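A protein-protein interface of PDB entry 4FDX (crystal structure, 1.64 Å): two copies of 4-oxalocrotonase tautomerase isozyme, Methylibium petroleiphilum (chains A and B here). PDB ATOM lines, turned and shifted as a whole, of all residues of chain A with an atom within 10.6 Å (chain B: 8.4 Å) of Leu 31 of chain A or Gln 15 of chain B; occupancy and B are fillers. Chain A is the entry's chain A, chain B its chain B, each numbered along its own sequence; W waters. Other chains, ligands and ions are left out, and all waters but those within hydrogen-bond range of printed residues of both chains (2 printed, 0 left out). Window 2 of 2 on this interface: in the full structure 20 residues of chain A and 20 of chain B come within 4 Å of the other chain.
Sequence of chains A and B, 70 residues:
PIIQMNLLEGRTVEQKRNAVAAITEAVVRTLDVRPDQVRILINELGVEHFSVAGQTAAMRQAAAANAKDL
The backbone NH (N) of Asn 6 of chain B is in hydrogen-bond range of the backbone carbonyl oxygen (O) of Ile 2 of chain A, 2.8 Å away.
O of Leu 31 of chain A is in hydrogen-bond range of NH1 of Arg 11 of chain B.
Of the printed residues of chain B, Arg 29 of chain A touches Ala 22.
Of the printed residues of chain B, Thr 30 of chain A touches Gln 15 (3.7 Å), Asn 18 (3.6 Å), Ala 19 (3.4 Å) and Ala 22 (3.7 Å).
Leu 31 of chain A touches just these residues of chain B: Leu 7, Arg 11, Gln 15 and Ala 19.
Printed residues of chain A within 4 Å of Met 5 of chain B: Ile 2 (3.6 Å).
Arg 11 of chain B touches two residues of chain A.
Gln 15 of chain B touches two residues of chain A.
Asn 18 of chain B touches one residue of chain A.
Of chain A, only Thr 30 (3.4 Å) and Leu 31 (3.9 Å) come within 4 Å of Ala 19 of chain B.
Of the printed residues of chain A, Ala 22 of chain B touches Ala 26, Arg 29 and Thr 30.
Printed residues of chain A within 4 Å of Ile 23 of chain B: Val 27 (3.8 Å).
The nearest residue of chain A that does not touch Gln 15 of chain B is Asp 32 of chain A (5.0 Å).
The nearest printed residue of chain B that does not touch Ile 2 of chain A is Leu 7 of chain B (5.3 Å).
Hydrophobic or aromatic side chains of chain B within 4 Å of the printed part of chain A: Leu 7, Ala 19, Ala 22 and Ile 23.
Along chain B the printed residues that touch a printed residue of chain A span positions 5 to 23.
Hydrophobic or aromatic side chains of chain A within 4 Å of the printed part of chain B: Pro 1, Ala 26, Val 27, Leu 31 and Val 33.
Among the printed residues, no Asp or Glu carboxylate lies within 4 Å of a Lys or Arg side-chain nitrogen of the other chain.
Water W2 bridges the backbone carbonyl oxygen of Thr 30 of chain A (2.7 Å) and the side-chain amide nitrogen of Asn 18 of chain B (3.0 Å).
Water W1 lies within hydrogen-bond range of O of Asn 18 of chain B (3.0 Å) and NH2 of Arg 29 of chain A (3.5 Å).
Pro 1 of chain A touches Asn 6 of chain B.
Pro 1 of chain A touches Leu 7 of chain B (CB to CD2, 3.9 Å).
Ile 2 of chain A touches Met 5 of chain B.
NH2 of Arg 29 of chain A touches CB of Ala 22 of chain B, 3.7 Å away.
CG of Gln 15 of chain B touches O of Thr 30 of chain A (3.7 Å).
Thr 30 of chain A touches Asn 18 of chain B (CG2 to O, 3.6 Å).
Ala 22 of chain B touches Thr 30 of chain A (CB to CG2, 3.7 Å).
CD2 of Leu 7 of chain B touches CD1 of Leu 31 of chain A (3.6 Å).
CB of Ala 19 of chain B touches CD2 of Leu 31 of chain A (3.9 Å).
Arg 11 of chain B touches Val 33 of chain A (NH2 to CG1, 3.4 Å).
O of Pro 1 of chain A sits at hydrogen-bond distance from N of Arg 39 of chain A (3.0 Å).
The side-chain hydroxyl (OG1) of Thr 30 of chain A lies within hydrogen-bond range of the backbone carbonyl oxygen (O) of Ala 26 of chain A, 2.8 Å away.
NH1 of Arg 11 of chain B lies close to NE2 of Gln 15 of chain B, at 3.3 Å.
The backbone NH of Thr 12 of chain B lies within hydrogen-bond range of the side-chain amide oxygen of Gln 15 of chain B, 3.3 Å away.
ND2 of Asn 18 of chain B lies close to O of Glu 14 of chain B, at 3.3 Å.
1 position is printed for both chains.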
ATOM      1  N   PRO A   1      19.586 -32.917  -7.207  1.00  0.00           N
ATOM      2  CA  PRO A   1      18.916 -31.856  -6.419  1.00  0.00           C
ATOM      3  C   PRO A   1      17.430 -32.041  -6.467  1.00  0.00           C
ATOM      4  O   PRO A   1      16.839 -32.338  -7.510  1.00  0.00           O
ATOM      5  CB  PRO A   1      19.391 -30.546  -7.089  1.00  0.00           C
ATOM      6  CG  PRO A   1      20.730 -30.956  -7.692  1.00  0.00           C
ATOM      7  CD  PRO A   1      20.643 -32.380  -8.100  1.00  0.00           C
ATOM      8  N   ILE A   2      16.768 -31.749  -5.365  1.00  0.00           N
ATOM      9  CA  ILE A   2      15.332 -31.846  -5.261  1.00  0.00           C
ATOM     10  C   ILE A   2      14.899 -30.424  -4.884  1.00  0.00           C
ATOM     11  O   ILE A   2      15.380 -29.852  -3.871  1.00  0.00           O
ATOM     12  CB  ILE A   2      14.909 -32.875  -4.212  1.00  0.00           C
ATOM     13  CG1 ILE A   2      15.245 -34.295  -4.770  1.00  0.00           C
ATOM     14  CG2 ILE A   2      13.396 -32.796  -3.990  1.00  0.00           C
ATOM     15  CD1 ILE A   2      15.061 -35.422  -3.757  1.00  0.00           C
ATOM     16  N   ILE A   3      14.038 -29.819  -5.707  1.00  0.00           N
ATOM     17  CA  ILE A   3      13.659 -28.394  -5.506  1.00  0.00           C
ATOM     18  C   ILE A   3      12.182 -28.363  -5.225  1.00  0.00           C
ATOM     19  O   ILE A   3      11.406 -29.009  -5.896  1.00  0.00           O
ATOM     20  CB  ILE A   3      13.954 -27.647  -6.742  1.00  0.00           C
ATOM     21  CG1 ILE A   3      15.482 -27.636  -6.798  1.00  0.00           C
ATOM     22  CG2 ILE A   3      13.332 -26.235  -6.677  1.00  0.00           C
ATOM     23  CD1 ILE A   3      15.857 -27.265  -8.146  1.00  0.00           C
ATOM     24  N   ILE A  23      14.221 -23.553 -14.481  1.00  0.00           N
ATOM     25  CA  ILE A  23      14.940 -23.817 -13.219  1.00  0.00           C
ATOM     26  C   ILE A  23      15.843 -25.070 -13.393  1.00  0.00           C
ATOM     27  O   ILE A  23      17.013 -25.085 -12.883  1.00  0.00           O
ATOM     28  CB  ILE A  23      13.917 -24.075 -12.067  1.00  0.00           C
ATOM     29  CG1 ILE A  23      13.239 -22.747 -11.701  1.00  0.00           C
ATOM     30  CG2 ILE A  23      14.622 -24.747 -10.880  1.00  0.00           C
ATOM     31  CD1 ILE A  23      11.958 -22.975 -10.872  1.00  0.00           C
ATOM     32  N   THR A  24      15.330 -26.107 -14.083  1.00  0.00           N
ATOM     33  CA  THR A  24      16.173 -27.306 -14.357  1.00  0.00           C
ATOM     34  C   THR A  24      17.422 -26.937 -15.112  1.00  0.00           C
ATOM     35  O   THR A  24      18.498 -27.324 -14.723  1.00  0.00           O
ATOM     36  CB  THR A  24      15.368 -28.396 -15.053  1.00  0.00           C
ATOM     37  OG1 THR A  24      14.265 -28.723 -14.151  1.00  0.00           O
ATOM     38  CG2 THR A  24      16.289 -29.652 -15.261  1.00  0.00           C
ATOM     39  N   GLU A  25      17.278 -26.112 -16.145  1.00  0.00           N
ATOM     40  CA  GLU A  25      18.447 -25.685 -16.948  1.00  0.00           C
ATOM     41  C   GLU A  25      19.439 -24.943 -16.101  1.00  0.00           C
ATOM     42  O   GLU A  25      20.633 -25.120 -16.192  1.00  0.00           O
ATOM     43  CB  GLU A  25      17.935 -24.858 -18.124  1.00  0.00           C
ATOM     44  CG  GLU A  25      17.208 -25.690 -19.176  1.00  0.00           C
ATOM     45  CD  GLU A  25      16.332 -24.868 -20.124  1.00  0.00           C
ATOM     46  OE1 GLU A  25      16.130 -23.669 -19.936  1.00  0.00           O
ATOM     47  OE2 GLU A  25      15.715 -25.492 -21.000  1.00  0.00           O
ATOM     48  N   ALA A  26      18.973 -24.055 -15.207  1.00  0.00           N
ATOM     49  CA  ALA A  26      19.834 -23.344 -14.278  1.00  0.00           C
ATOM     50  C   ALA A  26      20.626 -24.250 -13.358  1.00  0.00           C
ATOM     51  O   ALA A  26      21.806 -24.020 -13.175  1.00  0.00           O
ATOM     52  CB  ALA A  26      19.000 -22.350 -13.451  1.00  0.00           C
ATOM     53  N   VAL A  27      19.990 -25.311 -12.851  1.00  0.00           N
ATOM     54  CA  VAL A  27      20.607 -26.265 -11.860  1.00  0.00           C
ATOM     55  C   VAL A  27      21.606 -27.099 -12.631  1.00  0.00           C
ATOM     56  O   VAL A  27      22.725 -27.230 -12.226  1.00  0.00           O
ATOM     57  CB  VAL A  27      19.494 -27.099 -11.211  1.00  0.00           C
ATOM     58  CG1 VAL A  27      20.165 -28.145 -10.306  1.00  0.00           C
ATOM     59  CG2 VAL A  27      18.654 -26.149 -10.311  1.00  0.00           C
ATOM     60  N   VAL A  28      21.238 -27.590 -13.779  1.00  0.00           N
ATOM     61  CA  VAL A  28      22.137 -28.396 -14.635  1.00  0.00           C
ATOM     62  C   VAL A  28      23.386 -27.600 -14.989  1.00  0.00           C
ATOM     63  O   VAL A  28      24.503 -28.117 -14.825  1.00  0.00           O
ATOM     64  CB  VAL A  28      21.395 -28.850 -15.901  1.00  0.00           C
ATOM     65  CG1 VAL A  28      22.435 -29.452 -16.904  1.00  0.00           C
ATOM     66  CG2 VAL A  28      20.435 -29.954 -15.552  1.00  0.00           C
ATOM     67  N   ARG A  29      23.207 -26.324 -15.390  1.00  0.00           N
ATOM     68  CA  ARG A  29      24.420 -25.514 -15.718  1.00  0.00           C
ATOM     69  C   ARG A  29      25.315 -25.199 -14.586  1.00  0.00           C
ATOM     70  O   ARG A  29      26.540 -25.303 -14.682  1.00  0.00           O
ATOM     71  CB  ARG A  29      24.025 -24.312 -16.557  1.00  0.00           C
ATOM     72  CG  ARG A  29      25.246 -23.483 -16.929  1.00  0.00           C
ATOM     73  CD  ARG A  29      24.742 -22.263 -17.774  1.00  0.00           C
ATOM     74  NE  ARG A  29      23.954 -21.318 -16.935  1.00  0.00           N
ATOM     75  CZ  ARG A  29      24.476 -20.440 -16.081  1.00  0.00           C
ATOM     76  NH1 ARG A  29      25.801 -20.395 -15.836  1.00  0.00           N
ATOM     77  NH2 ARG A  29      23.648 -19.705 -15.342  1.00  0.00           N
ATOM     78  N   THR A  30      24.742 -24.725 -13.469  1.00  0.00           N
ATOM     79  CA  THR A  30      25.465 -24.178 -12.367  1.00  0.00           C
ATOM     80  C   THR A  30      26.078 -25.241 -11.449  1.00  0.00           C
ATOM     81  O   THR A  30      27.071 -24.979 -10.723  1.00  0.00           O
ATOM     82  CB  THR A  30      24.653 -23.160 -11.530  1.00  0.00           C
ATOM     83  OG1 THR A  30      23.491 -23.812 -10.998  1.00  0.00           O
ATOM     84  CG2 THR A  30      24.294 -21.879 -12.354  1.00  0.00           C
ATOM     85  N   LEU A  31      25.386 -26.393 -11.323  1.00  0.00           N
ATOM     86  CA  LEU A  31      25.897 -27.458 -10.442  1.00  0.00           C
ATOM     87  C   LEU A  31      26.541 -28.624 -11.250  1.00  0.00           C
ATOM     88  O   LEU A  31      27.039 -29.630 -10.621  1.00  0.00           O
ATOM     89  CB  LEU A  31      24.696 -28.028  -9.647  1.00  0.00           C
ATOM     90  CG  LEU A  31      24.019 -27.050  -8.668  1.00  0.00           C
ATOM     91  CD1 LEU A  31      23.027 -27.737  -7.709  1.00  0.00           C
ATOM     92  CD2 LEU A  31      24.977 -26.219  -7.841  1.00  0.00           C
ATOM     93  N   ASP A  32      26.455 -28.592 -12.562  1.00  0.00           N
ATOM     94  CA  ASP A  32      26.947 -29.695 -13.462  1.00  0.00           C
ATOM     95  C   ASP A  32      26.445 -31.099 -12.982  1.00  0.00           C
ATOM     96  O   ASP A  32      27.202 -32.021 -12.484  1.00  0.00           O
ATOM     97  CB  ASP A  32      28.456 -29.593 -13.835  1.00  0.00           C
ATOM     98  CG  ASP A  32      28.822 -30.369 -15.213  1.00  0.00           C
ATOM     99  OD1 ASP A  32      29.750 -31.186 -15.125  1.00  0.00           O
ATOM    100  OD2 ASP A  32      28.212 -30.236 -16.368  1.00  0.00           O
ATOM    101  N   VAL A  33      25.115 -31.196 -12.977  1.00  0.00           N
ATOM    102  CA  VAL A  33      24.401 -32.458 -12.801  1.00  0.00           C
ATOM    103  C   VAL A  33      23.612 -32.716 -14.047  1.00  0.00           C
ATOM    104  O   VAL A  33      23.392 -31.832 -14.916  1.00  0.00           O
ATOM    105  CB  VAL A  33      23.444 -32.382 -11.586  1.00  0.00           C
ATOM    106  CG1 VAL A  33      24.249 -32.182 -10.360  1.00  0.00           C
ATOM    107  CG2 VAL A  33      22.444 -31.221 -11.759  1.00  0.00           C
ATOM    108  N   ARG A  34      23.229 -33.988 -14.238  1.00  0.00           N
ATOM    109  CA  ARG A  34      22.358 -34.355 -15.332  1.00  0.00           C
ATOM    110  C   ARG A  34      20.933 -33.851 -15.126  1.00  0.00           C
ATOM    111  O   ARG A  34      20.447 -33.757 -13.978  1.00  0.00           O
ATOM    112  CB  ARG A  34      22.308 -35.906 -15.523  1.00  0.00           C
ATOM    113  CG  ARG A  34      23.632 -36.623 -15.586  1.00  0.00           C
ATOM    114  CD  ARG A  34      23.404 -38.095 -16.008  1.00  0.00           C
ATOM    115  NE  ARG A  34      22.422 -38.729 -15.114  1.00  0.00           N
ATOM    116  CZ  ARG A  34      22.806 -39.416 -14.037  1.00  0.00           C
ATOM    117  NH1 ARG A  34      24.120 -39.505 -13.718  1.00  0.00           N
ATOM    118  NH2 ARG A  34      21.921 -39.964 -13.235  1.00  0.00           N
ATOM    119  N   PRO A  35      20.205 -33.555 -16.196  1.00  0.00           N
ATOM    120  CA  PRO A  35      18.753 -33.264 -16.073  1.00  0.00           C
ATOM    121  C   PRO A  35      17.981 -34.257 -15.267  1.00  0.00           C
ATOM    122  O   PRO A  35      17.093 -33.861 -14.460  1.00  0.00           O
ATOM    123  CB  PRO A  35      18.245 -33.246 -17.509  1.00  0.00           C
ATOM    124  CG  PRO A  35      19.506 -32.785 -18.253  1.00  0.00           C
ATOM    125  CD  PRO A  35      20.711 -33.338 -17.588  1.00  0.00           C
ATOM    126  N   GLN A  37      18.796 -35.781 -12.758  1.00  0.00           N
ATOM    127  CA  GLN A  37      19.098 -35.710 -11.299  1.00  0.00           C
ATOM    128  C   GLN A  37      18.347 -34.510 -10.703  1.00  0.00           C
ATOM    129  O   GLN A  37      18.467 -34.281  -9.512  1.00  0.00           O
ATOM    130  CB  GLN A  37      20.606 -35.508 -11.037  1.00  0.00           C
ATOM    131  CG  GLN A  37      21.353 -36.792 -11.469  1.00  0.00           C
ATOM    132  CD  GLN A  37      22.871 -36.629 -11.357  1.00  0.00           C
ATOM    133  OE1 GLN A  37      23.517 -35.832 -12.032  1.00  0.00           O
ATOM    134  NE2 GLN A  37      23.447 -37.440 -10.475  1.00  0.00           N
ATOM    135  N   VAL A  38      17.605 -33.781 -11.498  1.00  0.00           N
ATOM    136  CA  VAL A  38      16.892 -32.584 -10.953  1.00  0.00           C
ATOM    137  C   VAL A  38      15.394 -32.826 -10.910  1.00  0.00           C
ATOM    138  O   VAL A  38      14.749 -33.082 -11.965  1.00  0.00           O
ATOM    139  CB  VAL A  38      17.198 -31.348 -11.873  1.00  0.00           C
ATOM    140  CG1 VAL A  38      16.448 -30.098 -11.362  1.00  0.00           C
ATOM    141  CG2 VAL A  38      18.734 -31.188 -11.947  1.00  0.00           C
ATOM    142  N   ARG A  39      14.854 -32.803  -9.706  1.00  0.00           N
ATOM    143  CA  ARG A  39      13.414 -32.997  -9.549  1.00  0.00           C
ATOM    144  C   ARG A  39      12.828 -31.735  -8.946  1.00  0.00           C
ATOM    145  O   ARG A  39      13.408 -31.117  -8.086  1.00  0.00           O
ATOM    146  CB  ARG A  39      13.165 -34.168  -8.641  1.00  0.00           C
ATOM    147  CG  ARG A  39      13.327 -35.488  -9.393  1.00  0.00           C
ATOM    148  CD  ARG A  39      13.457 -36.675  -8.429  1.00  0.00           C
ATOM    149  NE  ARG A  39      13.381 -37.879  -9.268  1.00  0.00           N
ATOM    150  CZ  ARG A  39      14.400 -38.237 -10.041  1.00  0.00           C
ATOM    151  NH1 ARG A  39      15.559 -37.599  -9.985  1.00  0.00           N
ATOM    152  NH2 ARG A  39      14.286 -39.263 -10.869  1.00  0.00           N
ATOM    153  N   MET B   5      15.908 -25.824  -1.930  1.00  0.00           N
ATOM    154  CA  MET B   5      16.751 -26.678  -2.759  1.00  0.00           C
ATOM    155  C   MET B   5      17.497 -27.605  -1.818  1.00  0.00           C
ATOM    156  O   MET B   5      18.276 -27.176  -1.001  1.00  0.00           O
ATOM    157  CB  MET B   5      17.660 -25.801  -3.605  1.00  0.00           C
ATOM    158  CG  MET B   5      18.660 -26.772  -4.267  1.00  0.00           C
ATOM    159  SD  MET B   5      19.483 -25.994  -5.682  1.00  0.00           S
ATOM    160  CE  MET B   5      20.394 -24.753  -4.899  1.00  0.00           C
ATOM    161  N   ASN B   6      17.283 -28.913  -2.009  1.00  0.00           N
ATOM    162  CA  ASN B   6      17.977 -29.956  -1.210  1.00  0.00           C
ATOM    163  C   ASN B   6      19.073 -30.528  -2.117  1.00  0.00           C
ATOM    164  O   ASN B   6      18.773 -30.959  -3.264  1.00  0.00           O
ATOM    165  CB  ASN B   6      16.948 -31.042  -0.848  1.00  0.00           C
ATOM    166  CG  ASN B   6      15.719 -30.482  -0.113  1.00  0.00           C
ATOM    167  OD1 ASN B   6      15.735 -30.275   1.079  1.00  0.00           O
ATOM    168  ND2 ASN B   6      14.646 -30.190  -0.859  1.00  0.00           N
ATOM    169  N   LEU B   7      20.306 -30.469  -1.608  1.00  0.00           N
ATOM    170  CA  LEU B   7      21.536 -30.815  -2.343  1.00  0.00           C
ATOM    171  C   LEU B   7      22.289 -31.725  -1.469  1.00  0.00           C
ATOM    172  O   LEU B   7      22.334 -31.487  -0.267  1.00  0.00           O
ATOM    173  CB  LEU B   7      22.576 -29.605  -2.455  1.00  0.00           C
ATOM    174  CG  LEU B   7      22.202 -28.324  -3.124  1.00  0.00           C
ATOM    175  CD1 LEU B   7      23.408 -27.440  -3.273  1.00  0.00           C
ATOM    176  CD2 LEU B   7      21.783 -28.754  -4.514  1.00  0.00           C
ATOM    177  N   LEU B   8      23.034 -32.677  -2.062  1.00  0.00           N
ATOM    178  CA  LEU B   8      24.105 -33.335  -1.279  1.00  0.00           C
ATOM    179  C   LEU B   8      25.222 -32.362  -0.855  1.00  0.00           C
ATOM    180  O   LEU B   8      25.526 -31.406  -1.608  1.00  0.00           O
ATOM    181  CB  LEU B   8      24.784 -34.467  -2.071  1.00  0.00           C
ATOM    182  CG  LEU B   8      23.945 -35.640  -2.384  1.00  0.00           C
ATOM    183  CD1 LEU B   8      24.756 -36.598  -3.279  1.00  0.00           C
ATOM    184  CD2 LEU B   8      23.681 -36.336  -1.063  1.00  0.00           C
ATOM    185  N   GLY B  10      28.974 -30.772   0.179  1.00  0.00           N
ATOM    186  CA  GLY B  10      30.276 -30.792  -0.492  1.00  0.00           C
ATOM    187  C   GLY B  10      30.513 -29.788  -1.579  1.00  0.00           C
ATOM    188  O   GLY B  10      31.668 -29.607  -1.952  1.00  0.00           O
ATOM    189  N   ARG B  11      29.461 -29.119  -2.078  1.00  0.00           N
ATOM    190  CA  ARG B  11      29.608 -28.059  -3.145  1.00  0.00           C
ATOM    191  C   ARG B  11      30.270 -26.793  -2.680  1.00  0.00           C
ATOM    192  O   ARG B  11      30.144 -26.399  -1.514  1.00  0.00           O
ATOM    193  CB  ARG B  11      28.259 -27.698  -3.702  1.00  0.00           C
ATOM    194  CG  ARG B  11      27.665 -28.980  -4.153  1.00  0.00           C
ATOM    195  CD  ARG B  11      26.896 -28.666  -5.338  1.00  0.00           C
ATOM    196  NE  ARG B  11      26.370 -29.871  -5.960  1.00  0.00           N
ATOM    197  CZ  ARG B  11      26.719 -30.278  -7.173  1.00  0.00           C
ATOM    198  NH1 ARG B  11      27.668 -29.627  -7.879  1.00  0.00           N
ATOM    199  NH2 ARG B  11      26.140 -31.363  -7.673  1.00  0.00           N
ATOM    200  N   THR B  12      30.971 -26.157  -3.614  1.00  0.00           N
ATOM    201  CA  THR B  12      31.744 -24.964  -3.233  1.00  0.00           C
ATOM    202  C   THR B  12      30.742 -23.776  -3.169  1.00  0.00           C
ATOM    203  O   THR B  12      29.649 -23.816  -3.811  1.00  0.00           O
ATOM    204  CB  THR B  12      33.124 -24.817  -4.014  1.00  0.00           C
ATOM    205  OG1 THR B  12      32.910 -25.205  -5.365  1.00  0.00           O
ATOM    206  CG2 THR B  12      34.504 -25.788  -3.414  1.00  0.00           C
ATOM    207  N   VAL B  13      31.031 -22.831  -2.312  1.00  0.00           N
ATOM    208  CA  VAL B  13      30.245 -21.638  -2.122  1.00  0.00           C
ATOM    209  C   VAL B  13      29.954 -20.997  -3.467  1.00  0.00           C
ATOM    210  O   VAL B  13      28.835 -20.510  -3.671  1.00  0.00           O
ATOM    211  CB  VAL B  13      30.984 -20.636  -1.159  1.00  0.00           C
ATOM    212  CG1 VAL B  13      30.458 -19.234  -1.353  1.00  0.00           C
ATOM    213  CG2 VAL B  13      30.686 -21.040   0.269  1.00  0.00           C
ATOM    214  N   GLU B  14      30.955 -20.914  -4.348  1.00  0.00           N
ATOM    215  CA  GLU B  14      30.713 -20.307  -5.685  1.00  0.00           C
ATOM    216  C   GLU B  14      29.617 -20.980  -6.453  1.00  0.00           C
ATOM    217  O   GLU B  14      28.796 -20.273  -7.055  1.00  0.00           O
ATOM    218  CB  GLU B  14      31.938 -20.359  -6.591  1.00  0.00           C
ATOM    219  CG  GLU B  14      32.952 -19.289  -6.306  1.00  0.00           C
ATOM    220  CD  GLU B  14      33.941 -19.668  -5.198  1.00  0.00           C
ATOM    221  OE1 GLU B  14      33.886 -20.802  -4.645  1.00  0.00           O
ATOM    222  OE2 GLU B  14      34.736 -18.767  -4.847  1.00  0.00           O
ATOM    223  N   GLN B  15      29.557 -22.304  -6.431  1.00  0.00           N
ATOM    224  CA  GLN B  15      28.529 -23.009  -7.187  1.00  0.00           C
ATOM    225  C   GLN B  15      27.166 -22.742  -6.568  1.00  0.00           C
ATOM    226  O   GLN B  15      26.191 -22.504  -7.270  1.00  0.00           O
ATOM    227  CB  GLN B  15      28.763 -24.529  -7.111  1.00  0.00           C
ATOM    228  CG  GLN B  15      29.697 -25.045  -8.132  1.00  0.00           C
ATOM    229  CD  GLN B  15      29.976 -26.520  -7.919  1.00  0.00           C
ATOM    230  OE1 GLN B  15      30.373 -26.941  -6.810  1.00  0.00           O
ATOM    231  NE2 GLN B  15      29.744 -27.317  -8.965  1.00  0.00           N
ATOM    232  N   LYS B  16      27.094 -22.754  -5.244  1.00  0.00           N
ATOM    233  CA  LYS B  16      25.810 -22.437  -4.531  1.00  0.00           C
ATOM    234  C   LYS B  16      25.389 -21.012  -4.926  1.00  0.00           C
ATOM    235  O   LYS B  16      24.199 -20.748  -5.169  1.00  0.00           O
ATOM    236  CB  LYS B  16      25.998 -22.576  -3.002  1.00  0.00           C
ATOM    237  CG  LYS B  16      26.165 -24.036  -2.529  1.00  0.00           C
ATOM    238  CD  LYS B  16      26.686 -23.934  -1.108  1.00  0.00           C
ATOM    239  CE  LYS B  16      26.870 -25.262  -0.442  1.00  0.00           C
ATOM    240  NZ  LYS B  16      27.238 -25.010   0.968  1.00  0.00           N
ATOM    241  N   ARG B  17      26.320 -20.042  -4.922  1.00  0.00           N
ATOM    242  CA  ARG B  17      25.977 -18.641  -5.254  1.00  0.00           C
ATOM    243  C   ARG B  17      25.518 -18.555  -6.715  1.00  0.00           C
ATOM    244  O   ARG B  17      24.510 -17.863  -7.009  1.00  0.00           O
ATOM    245  CB  ARG B  17      27.201 -17.751  -5.061  1.00  0.00           C
ATOM    246  CG  ARG B  17      27.477 -17.452  -3.556  1.00  0.00           C
ATOM    247  CD  ARG B  17      28.612 -16.429  -3.517  1.00  0.00           C
ATOM    248  NE  ARG B  17      29.132 -16.405  -2.167  1.00  0.00           N
ATOM    249  CZ  ARG B  17      30.419 -16.061  -1.911  1.00  0.00           C
ATOM    250  NH1 ARG B  17      31.242 -15.711  -2.929  1.00  0.00           N
ATOM    251  NH2 ARG B  17      30.910 -16.105  -0.657  1.00  0.00           N
ATOM    252  N   ASN B  18      26.198 -19.251  -7.612  1.00  0.00           N
ATOM    253  CA  ASN B  18      25.737 -19.226  -9.030  1.00  0.00           C
ATOM    254  C   ASN B  18      24.366 -19.871  -9.174  1.00  0.00           C
ATOM    255  O   ASN B  18      23.545 -19.312  -9.885  1.00  0.00           O
ATOM    256  CB  ASN B  18      26.739 -19.937  -9.963  1.00  0.00           C
ATOM    257  CG  ASN B  18      28.092 -19.197 -10.011  1.00  0.00           C
ATOM    258  OD1 ASN B  18      28.162 -17.980  -9.824  1.00  0.00           O
ATOM    259  ND2 ASN B  18      29.196 -19.968 -10.344  1.00  0.00           N
ATOM    260  N   ALA B  19      24.132 -20.996  -8.474  1.00  0.00           N
ATOM    261  CA  ALA B  19      22.775 -21.594  -8.528  1.00  0.00           C
ATOM    262  C   ALA B  19      21.696 -20.645  -8.025  1.00  0.00           C
ATOM    263  O   ALA B  19      20.638 -20.573  -8.622  1.00  0.00           O
ATOM    264  CB  ALA B  19      22.806 -22.922  -7.725  1.00  0.00           C
ATOM    265  N   VAL B  20      21.928 -20.002  -6.911  1.00  0.00           N
ATOM    266  CA  VAL B  20      20.950 -19.087  -6.324  1.00  0.00           C
ATOM    267  C   VAL B  20      20.662 -17.928  -7.331  1.00  0.00           C
ATOM    268  O   VAL B  20      19.503 -17.553  -7.557  1.00  0.00           O
ATOM    269  CB  VAL B  20      21.591 -18.531  -4.984  1.00  0.00           C
ATOM    270  CG1 VAL B  20      21.052 -17.140  -4.603  1.00  0.00           C
ATOM    271  CG2 VAL B  20      21.431 -19.655  -3.913  1.00  0.00           C
ATOM    272  N   ALA B  21      21.671 -17.356  -7.951  1.00  0.00           N
ATOM    273  CA  ALA B  21      21.391 -16.335  -8.956  1.00  0.00           C
ATOM    274  C   ALA B  21      20.661 -16.833 -10.187  1.00  0.00           C
ATOM    275  O   ALA B  21      19.721 -16.172 -10.614  1.00  0.00           O
ATOM    276  CB  ALA B  21      22.753 -15.706  -9.371  1.00  0.00           C
ATOM    277  N   ALA B  22      21.041 -18.014 -10.693  1.00  0.00           N
ATOM    278  CA  ALA B  22      20.458 -18.554 -11.885  1.00  0.00           C
ATOM    279  C   ALA B  22      19.030 -18.995 -11.638  1.00  0.00           C
ATOM    280  O   ALA B  22      18.135 -18.712 -12.436  1.00  0.00           O
ATOM    281  CB  ALA B  22      21.353 -19.691 -12.379  1.00  0.00           C
ATOM    282  N   ILE B  23      18.803 -19.636 -10.489  1.00  0.00           N
ATOM    283  CA  ILE B  23      17.404 -20.049 -10.166  1.00  0.00           C
ATOM    284  C   ILE B  23      16.519 -18.827 -10.012  1.00  0.00           C
ATOM    285  O   ILE B  23      15.374 -18.787 -10.486  1.00  0.00           O
ATOM    286  CB  ILE B  23      17.349 -20.984  -8.901  1.00  0.00           C
ATOM    287  CG1 ILE B  23      18.022 -22.317  -9.245  1.00  0.00           C
ATOM    288  CG2 ILE B  23      15.893 -21.200  -8.422  1.00  0.00           C
ATOM    289  CD1 ILE B  23      18.348 -23.188  -8.009  1.00  0.00           C
ATOM    290  N   ILE B  42      18.616 -23.246   1.032  1.00  0.00           N
ATOM    291  CA  ILE B  42      19.412 -24.428   0.624  1.00  0.00           C
ATOM    292  C   ILE B  42      19.565 -25.313   1.808  1.00  0.00           C
ATOM    293  O   ILE B  42      19.985 -24.898   2.942  1.00  0.00           O
ATOM    294  CB  ILE B  42      20.799 -24.005   0.140  1.00  0.00           C
ATOM    295  CG1 ILE B  42      20.689 -23.261  -1.183  1.00  0.00           C
ATOM    296  CG2 ILE B  42      21.643 -25.235  -0.061  1.00  0.00           C
ATOM    297  CD1 ILE B  42      22.057 -22.632  -1.590  1.00  0.00           C
HETATM  298  O   HOH W   1      24.591 -18.153 -12.407  1.00  0.00           O
HETATM  299  O   HOH W   2      28.783 -22.888 -11.119  1.00  0.00           O
